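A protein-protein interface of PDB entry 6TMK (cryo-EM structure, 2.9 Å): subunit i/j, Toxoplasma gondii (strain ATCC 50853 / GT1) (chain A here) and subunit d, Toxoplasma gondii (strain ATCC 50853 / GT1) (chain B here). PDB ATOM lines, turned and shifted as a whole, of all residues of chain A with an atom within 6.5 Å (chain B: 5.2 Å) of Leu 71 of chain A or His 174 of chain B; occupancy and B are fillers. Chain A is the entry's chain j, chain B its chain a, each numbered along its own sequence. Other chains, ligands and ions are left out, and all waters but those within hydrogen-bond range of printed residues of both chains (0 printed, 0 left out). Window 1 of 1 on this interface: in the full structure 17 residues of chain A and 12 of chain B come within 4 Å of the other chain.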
ATOM      1  N   PRO A  68      -1.990   8.941 -26.498  1.00  0.00           N
ATOM      2  CA  PRO A  68      -1.888   9.723 -27.729  1.00  0.00           C
ATOM      3  C   PRO A  68      -1.572  11.187 -27.477  1.00  0.00           C
ATOM      4  O   PRO A  68      -1.822  11.740 -26.405  1.00  0.00           O
ATOM      5  CB  PRO A  68      -3.277   9.568 -28.352  1.00  0.00           C
ATOM      6  CG  PRO A  68      -4.165   9.323 -27.218  1.00  0.00           C
ATOM      7  CD  PRO A  68      -3.378   8.556 -26.211  1.00  0.00           C
ATOM      8  N   ASN A  69      -1.011  11.807 -28.506  1.00  0.00           N
ATOM      9  CA  ASN A  69      -0.728  13.235 -28.525  1.00  0.00           C
ATOM     10  C   ASN A  69      -1.532  13.840 -29.669  1.00  0.00           C
ATOM     11  O   ASN A  69      -1.080  13.862 -30.815  1.00  0.00           O
ATOM     12  CB  ASN A  69       0.748  13.471 -28.687  1.00  0.00           C
ATOM     13  CG  ASN A  69       1.146  14.887 -28.407  1.00  0.00           C
ATOM     14  OD1 ASN A  69       0.306  15.761 -28.210  1.00  0.00           O
ATOM     15  ND2 ASN A  69       2.441  15.130 -28.402  1.00  0.00           N
ATOM     16  N   PHE A  70      -2.731  14.326 -29.356  1.00  0.00           N
ATOM     17  CA  PHE A  70      -3.575  14.923 -30.379  1.00  0.00           C
ATOM     18  C   PHE A  70      -3.020  16.237 -30.904  1.00  0.00           C
ATOM     19  O   PHE A  70      -3.369  16.644 -32.015  1.00  0.00           O
ATOM     20  CB  PHE A  70      -4.980  15.128 -29.827  1.00  0.00           C
ATOM     21  CG  PHE A  70      -5.638  13.865 -29.371  1.00  0.00           C
ATOM     22  CD1 PHE A  70      -6.019  12.900 -30.279  1.00  0.00           C
ATOM     23  CD2 PHE A  70      -5.880  13.644 -28.036  1.00  0.00           C
ATOM     24  CE1 PHE A  70      -6.623  11.749 -29.860  1.00  0.00           C
ATOM     25  CE2 PHE A  70      -6.483  12.491 -27.618  1.00  0.00           C
ATOM     26  CZ  PHE A  70      -6.858  11.543 -28.533  1.00  0.00           C
ATOM     27  N   LEU A  71      -2.161  16.899 -30.135  1.00  0.00           N
ATOM     28  CA  LEU A  71      -1.520  18.128 -30.573  1.00  0.00           C
ATOM     29  C   LEU A  71      -0.356  17.881 -31.515  1.00  0.00           C
ATOM     30  O   LEU A  71       0.011  18.783 -32.274  1.00  0.00           O
ATOM     31  CB  LEU A  71      -1.050  18.931 -29.365  1.00  0.00           C
ATOM     32  CG  LEU A  71      -2.075  19.111 -28.254  1.00  0.00           C
ATOM     33  CD1 LEU A  71      -1.458  19.842 -27.098  1.00  0.00           C
ATOM     34  CD2 LEU A  71      -3.276  19.850 -28.768  1.00  0.00           C
ATOM     35  N   ARG A  72       0.227  16.690 -31.481  1.00  0.00           N
ATOM     36  CA  ARG A  72       1.340  16.332 -32.351  1.00  0.00           C
ATOM     37  C   ARG A  72       2.526  17.264 -32.135  1.00  0.00           C
ATOM     38  O   ARG A  72       3.236  17.631 -33.071  1.00  0.00           O
ATOM     39  CB  ARG A  72       0.908  16.327 -33.813  1.00  0.00           C
ATOM     40  CG  ARG A  72      -0.235  15.400 -34.106  1.00  0.00           C
ATOM     41  CD  ARG A  72       0.181  13.972 -33.966  1.00  0.00           C
ATOM     42  NE  ARG A  72      -0.731  13.052 -34.633  1.00  0.00           N
ATOM     43  CZ  ARG A  72      -1.760  12.448 -34.053  1.00  0.00           C
ATOM     44  NH1 ARG A  72      -2.048  12.651 -32.780  1.00  0.00           N
ATOM     45  NH2 ARG A  72      -2.515  11.636 -34.760  1.00  0.00           N
ATOM     46  N   GLN A  73       2.745  17.632 -30.879  1.00  0.00           N
ATOM     47  CA  GLN A  73       3.822  18.511 -30.470  1.00  0.00           C
ATOM     48  C   GLN A  73       4.401  17.987 -29.168  1.00  0.00           C
ATOM     49  O   GLN A  73       3.674  17.412 -28.351  1.00  0.00           O
ATOM     50  CB  GLN A  73       3.338  19.952 -30.259  1.00  0.00           C
ATOM     51  CG  GLN A  73       2.887  20.663 -31.504  1.00  0.00           C
ATOM     52  CD  GLN A  73       4.044  21.204 -32.295  1.00  0.00           C
ATOM     53  OE1 GLN A  73       5.112  20.598 -32.356  1.00  0.00           O
ATOM     54  NE2 GLN A  73       3.852  22.367 -32.885  1.00  0.00           N
ATOM     55  N   GLN A  78       4.971  22.534 -25.812  1.00  0.00           N
ATOM     56  CA  GLN A  78       3.739  22.962 -25.158  1.00  0.00           C
ATOM     57  C   GLN A  78       4.023  23.944 -24.027  1.00  0.00           C
ATOM     58  O   GLN A  78       3.369  24.987 -23.914  1.00  0.00           O
ATOM     59  CB  GLN A  78       2.979  21.754 -24.625  1.00  0.00           C
ATOM     60  CG  GLN A  78       2.543  20.775 -25.670  1.00  0.00           C
ATOM     61  CD  GLN A  78       1.817  19.594 -25.088  1.00  0.00           C
ATOM     62  OE1 GLN A  78       1.090  19.720 -24.107  1.00  0.00           O
ATOM     63  NE2 GLN A  78       2.005  18.434 -25.691  1.00  0.00           N
ATOM     64  N   VAL B 170      -7.521  21.767 -33.433  1.00  0.00           N
ATOM     65  CA  VAL B 170      -7.196  21.365 -32.073  1.00  0.00           C
ATOM     66  C   VAL B 170      -5.955  22.090 -31.573  1.00  0.00           C
ATOM     67  O   VAL B 170      -5.902  22.531 -30.421  1.00  0.00           O
ATOM     68  CB  VAL B 170      -7.018  19.837 -32.044  1.00  0.00           C
ATOM     69  CG1 VAL B 170      -6.413  19.363 -30.743  1.00  0.00           C
ATOM     70  CG2 VAL B 170      -8.331  19.163 -32.295  1.00  0.00           C
ATOM     71  N   GLU B 171      -4.939  22.209 -32.424  1.00  0.00           N
ATOM     72  CA  GLU B 171      -3.724  22.927 -32.060  1.00  0.00           C
ATOM     73  C   GLU B 171      -4.022  24.377 -31.691  1.00  0.00           C
ATOM     74  O   GLU B 171      -3.429  24.931 -30.754  1.00  0.00           O
ATOM     75  CB  GLU B 171      -2.745  22.851 -33.226  1.00  0.00           C
ATOM     76  CG  GLU B 171      -1.290  22.966 -32.876  1.00  0.00           C
ATOM     77  CD  GLU B 171      -0.426  23.167 -34.100  1.00  0.00           C
ATOM     78  OE1 GLU B 171      -0.985  23.227 -35.216  1.00  0.00           O
ATOM     79  OE2 GLU B 171       0.809  23.263 -33.952  1.00  0.00           O
ATOM     80  N   LYS B 172      -4.946  25.000 -32.424  1.00  0.00           N
ATOM     81  CA  LYS B 172      -5.269  26.405 -32.221  1.00  0.00           C
ATOM     82  C   LYS B 172      -5.805  26.674 -30.824  1.00  0.00           C
ATOM     83  O   LYS B 172      -5.484  27.699 -30.214  1.00  0.00           O
ATOM     84  CB  LYS B 172      -6.278  26.841 -33.272  1.00  0.00           C
ATOM     85  CG  LYS B 172      -6.479  28.320 -33.374  1.00  0.00           C
ATOM     86  CD  LYS B 172      -7.808  28.646 -33.980  1.00  0.00           C
ATOM     87  CE  LYS B 172      -8.164  30.086 -33.767  1.00  0.00           C
ATOM     88  NZ  LYS B 172      -8.822  30.674 -34.948  1.00  0.00           N
ATOM     89  N   HIS B 173      -6.623  25.769 -30.301  1.00  0.00           N
ATOM     90  CA  HIS B 173      -7.355  26.010 -29.070  1.00  0.00           C
ATOM     91  C   HIS B 173      -6.772  25.295 -27.865  1.00  0.00           C
ATOM     92  O   HIS B 173      -7.046  25.706 -26.734  1.00  0.00           O
ATOM     93  CB  HIS B 173      -8.818  25.594 -29.244  1.00  0.00           C
ATOM     94  CG  HIS B 173      -9.567  26.438 -30.221  1.00  0.00           C
ATOM     95  ND1 HIS B 173      -9.941  27.733 -29.943  1.00  0.00           N
ATOM     96  CD2 HIS B 173      -9.994  26.183 -31.478  1.00  0.00           C
ATOM     97  CE1 HIS B 173     -10.577  28.236 -30.984  1.00  0.00           C
ATOM     98  NE2 HIS B 173     -10.621  27.317 -31.929  1.00  0.00           N
ATOM     99  N   HIS B 174      -5.985  24.249 -28.074  1.00  0.00           N
ATOM    100  CA  HIS B 174      -5.525  23.402 -26.993  1.00  0.00           C
ATOM    101  C   HIS B 174      -4.014  23.274 -26.920  1.00  0.00           C
ATOM    102  O   HIS B 174      -3.503  22.785 -25.907  1.00  0.00           O
ATOM    103  CB  HIS B 174      -6.170  22.019 -27.112  1.00  0.00           C
ATOM    104  CG  HIS B 174      -7.654  22.058 -26.961  1.00  0.00           C
ATOM    105  ND1 HIS B 174      -8.517  21.716 -27.977  1.00  0.00           N
ATOM    106  CD2 HIS B 174      -8.428  22.450 -25.924  1.00  0.00           C
ATOM    107  CE1 HIS B 174      -9.760  21.871 -27.562  1.00  0.00           C
ATOM    108  NE2 HIS B 174      -9.733  22.315 -26.320  1.00  0.00           N
ATOM    109  N   PHE B 175      -3.291  23.702 -27.948  1.00  0.00           N
ATOM    110  CA  PHE B 175      -1.844  23.838 -27.900  1.00  0.00           C
ATOM    111  C   PHE B 175      -1.409  25.280 -27.741  1.00  0.00           C
ATOM    112  O   PHE B 175      -0.473  25.563 -26.990  1.00  0.00           O
ATOM    113  CB  PHE B 175      -1.210  23.262 -29.163  1.00  0.00           C
ATOM    114  CG  PHE B 175       0.237  23.594 -29.316  1.00  0.00           C
ATOM    115  CD1 PHE B 175       1.183  23.001 -28.515  1.00  0.00           C
ATOM    116  CD2 PHE B 175       0.653  24.502 -30.261  1.00  0.00           C
ATOM    117  CE1 PHE B 175       2.508  23.308 -28.656  1.00  0.00           C
ATOM    118  CE2 PHE B 175       1.975  24.810 -30.401  1.00  0.00           C
ATOM    119  CZ  PHE B 175       2.902  24.213 -29.599  1.00  0.00           C
ATOM    120  N   TYR B 176      -2.075  26.206 -28.423  1.00  0.00           N
ATOM    121  CA  TYR B 176      -1.733  27.611 -28.275  1.00  0.00           C
ATOM    122  C   TYR B 176      -2.391  28.244 -27.059  1.00  0.00           C
ATOM    123  O   TYR B 176      -1.993  29.344 -26.661  1.00  0.00           O
ATOM    124  CB  TYR B 176      -2.111  28.365 -29.542  1.00  0.00           C
ATOM    125  CG  TYR B 176      -1.186  28.069 -30.694  1.00  0.00           C
ATOM    126  CD1 TYR B 176       0.083  28.606 -30.740  1.00  0.00           C
ATOM    127  CD2 TYR B 176      -1.575  27.236 -31.723  1.00  0.00           C
ATOM    128  CE1 TYR B 176       0.930  28.335 -31.779  1.00  0.00           C
ATOM    129  CE2 TYR B 176      -0.734  26.959 -32.766  1.00  0.00           C
ATOM    130  CZ  TYR B 176       0.519  27.507 -32.789  1.00  0.00           C
ATOM    131  OH  TYR B 176       1.363  27.229 -33.835  1.00  0.00           O
ATOM    132  N   SER B 177      -3.376  27.578 -26.464  1.00  0.00           N
ATOM    133  CA  SER B 177      -3.966  27.994 -25.204  1.00  0.00           C
ATOM    134  C   SER B 177      -4.035  26.802 -24.262  1.00  0.00           C
ATOM    135  O   SER B 177      -3.922  25.646 -24.675  1.00  0.00           O
ATOM    136  CB  SER B 177      -5.362  28.582 -25.396  1.00  0.00           C
ATOM    137  OG  SER B 177      -5.789  29.262 -24.229  1.00  0.00           O
ATOM    138  N   GLN B 178      -4.231  27.104 -22.982  1.00  0.00           N
ATOM    139  CA  GLN B 178      -4.358  26.102 -21.937  1.00  0.00           C
ATOM    140  C   GLN B 178      -5.668  26.212 -21.176  1.00  0.00           C
ATOM    141  O   GLN B 178      -5.941  25.365 -20.321  1.00  0.00           O
ATOM    142  CB  GLN B 178      -3.200  26.205 -20.940  1.00  0.00           C
ATOM    143  CG  GLN B 178      -1.820  25.928 -21.492  1.00  0.00           C
ATOM    144  CD  GLN B 178      -1.545  24.457 -21.671  1.00  0.00           C
ATOM    145  OE1 GLN B 178      -1.201  24.006 -22.760  1.00  0.00           O
ATOM    146  NE2 GLN B 178      -1.704  23.695 -20.599  1.00  0.00           N
ATOM    147  N   GLN B 180      -8.872  27.000 -22.764  1.00  0.00           N
ATOM    148  CA  GLN B 180     -10.053  26.929 -23.601  1.00  0.00           C
ATOM    149  C   GLN B 180     -10.920  25.745 -23.183  1.00  0.00           C
ATOM    150  O   GLN B 180     -10.402  24.702 -22.779  1.00  0.00           O
ATOM    151  CB  GLN B 180      -9.665  26.793 -25.064  1.00  0.00           C
ATOM    152  CG  GLN B 180      -9.110  28.051 -25.681  1.00  0.00           C
ATOM    153  CD  GLN B 180     -10.162  29.107 -25.874  1.00  0.00           C
ATOM    154  OE1 GLN B 180     -10.487  29.856 -24.956  1.00  0.00           O
ATOM    155  NE2 GLN B 180     -10.706  29.172 -27.074  1.00  0.00           N
ATOM    156  N   PRO B 181     -12.238  25.873 -23.280  1.00  0.00           N
ATOM    157  CA  PRO B 181     -13.109  24.788 -22.828  1.00  0.00           C
ATOM    158  C   PRO B 181     -13.031  23.577 -23.739  1.00  0.00           C
ATOM    159  O   PRO B 181     -12.745  23.679 -24.934  1.00  0.00           O
ATOM    160  CB  PRO B 181     -14.501  25.419 -22.863  1.00  0.00           C
ATOM    161  CG  PRO B 181     -14.397  26.458 -23.903  1.00  0.00           C
ATOM    162  CD  PRO B 181     -13.017  27.011 -23.790  1.00  0.00           C
ATOM    163  N   GLY B 182     -13.295  22.415 -23.153  1.00  0.00           N
ATOM    164  CA  GLY B 182     -13.260  21.186 -23.913  1.00  0.00           C
ATOM    165  C   GLY B 182     -14.567  20.902 -24.612  1.00  0.00           C
ATOM    166  O   GLY B 182     -15.178  19.850 -24.404  1.00  0.00           O
ATOM    167  N   VAL B 183     -15.001  21.830 -25.454  1.00  0.00           N
ATOM    168  CA  VAL B 183     -16.233  21.676 -26.206  1.00  0.00           C
ATOM    169  C   VAL B 183     -15.871  21.474 -27.669  1.00  0.00           C
ATOM    170  O   VAL B 183     -14.762  21.780 -28.116  1.00  0.00           O
ATOM    171  CB  VAL B 183     -17.188  22.872 -26.027  1.00  0.00           C
ATOM    172  CG1 VAL B 183     -17.657  22.953 -24.600  1.00  0.00           C
ATOM    173  CG2 VAL B 183     -16.521  24.166 -26.434  1.00  0.00           C
ATOM    174  N   PRO B 186     -15.293  25.681 -29.872  1.00  0.00           N
ATOM    175  CA  PRO B 186     -15.001  26.851 -29.036  1.00  0.00           C
ATOM    176  C   PRO B 186     -15.120  28.180 -29.758  1.00  0.00           C
ATOM    177  O   PRO B 186     -15.157  29.221 -29.089  1.00  0.00           O
ATOM    178  CB  PRO B 186     -13.555  26.608 -28.586  1.00  0.00           C
ATOM    179  CG  PRO B 186     -13.240  25.222 -28.946  1.00  0.00           C
ATOM    180  CD  PRO B 186     -14.095  24.865 -30.093  1.00  0.00           C
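Leu 71 of chain A touches just these residues of chain B: Val 170, His 174 and Phe 175.
Printed residues of chain A within 4 Å of His 174 of chain B: Leu 71.
Of the printed residues of chain A, Val 170 of chain B touches Leu 71.
Of the printed residues of chain B, Gln 78 of chain A touches Phe 175.
Of the printed residues of chain A, Phe 175 of chain B touches Leu 71, Gln 73 and Gln 78.
The nearest printed residue of chain B that does not touch Gln 73 of chain A is Tyr 176 of chain B (5.5 Å).
Val 170 of chain B touches Leu 71 of chain A.
Leu 71 of chain A touches His 174 of chain B.
Phe 175 of chain B touches Leu 71 of chain A (N to CD2, 3.9 Å).
CB of Gln 73 of chain A touches CE1 of Phe 175 of chain B, at 3.8 Å.
Phe 175 of chain B touches Gln 78 of chain A (CE1 to CA, 3.7 Å).
The side-chain amide nitrogen (NE2) of Gln 73 of chain A lies within hydrogen-bond range of the side-chain carboxylate (OE2) of Glu 171 of chain B (3.3 Å).
N of Leu 71 of chain A lies close to OD1 of Asn 69 of chain A, 3.3 Å away.
O of Gln 73 of chain A sits at hydrogen-bond distance from NE2 of Gln 78 of chain A.
The backbone NH (N) of Tyr 176 of chain B sits at hydrogen-bond distance from the backbone carbonyl oxygen (O) of Glu 171 of chain B (3.0 Å).
The side-chain amide nitrogen (ND2) of Asn 69 of chain A lies within hydrogen-bond range of the backbone carbonyl oxygen (O) of Gln 73 of chain A (2.6 Å).
Of the 14 printed residues of chain B, 4 touch a printed residue of chain A.
Printed residues of chain B that touch a printed residue of chain A: Val 170, Glu 171, His 174 and Phe 175.
Hydrophobic or aromatic side chains of chain B that line the printed part of chain A: Val 170, His 174 and Phe 175.
Among the printed residues, 6 pairs touch across the chains.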
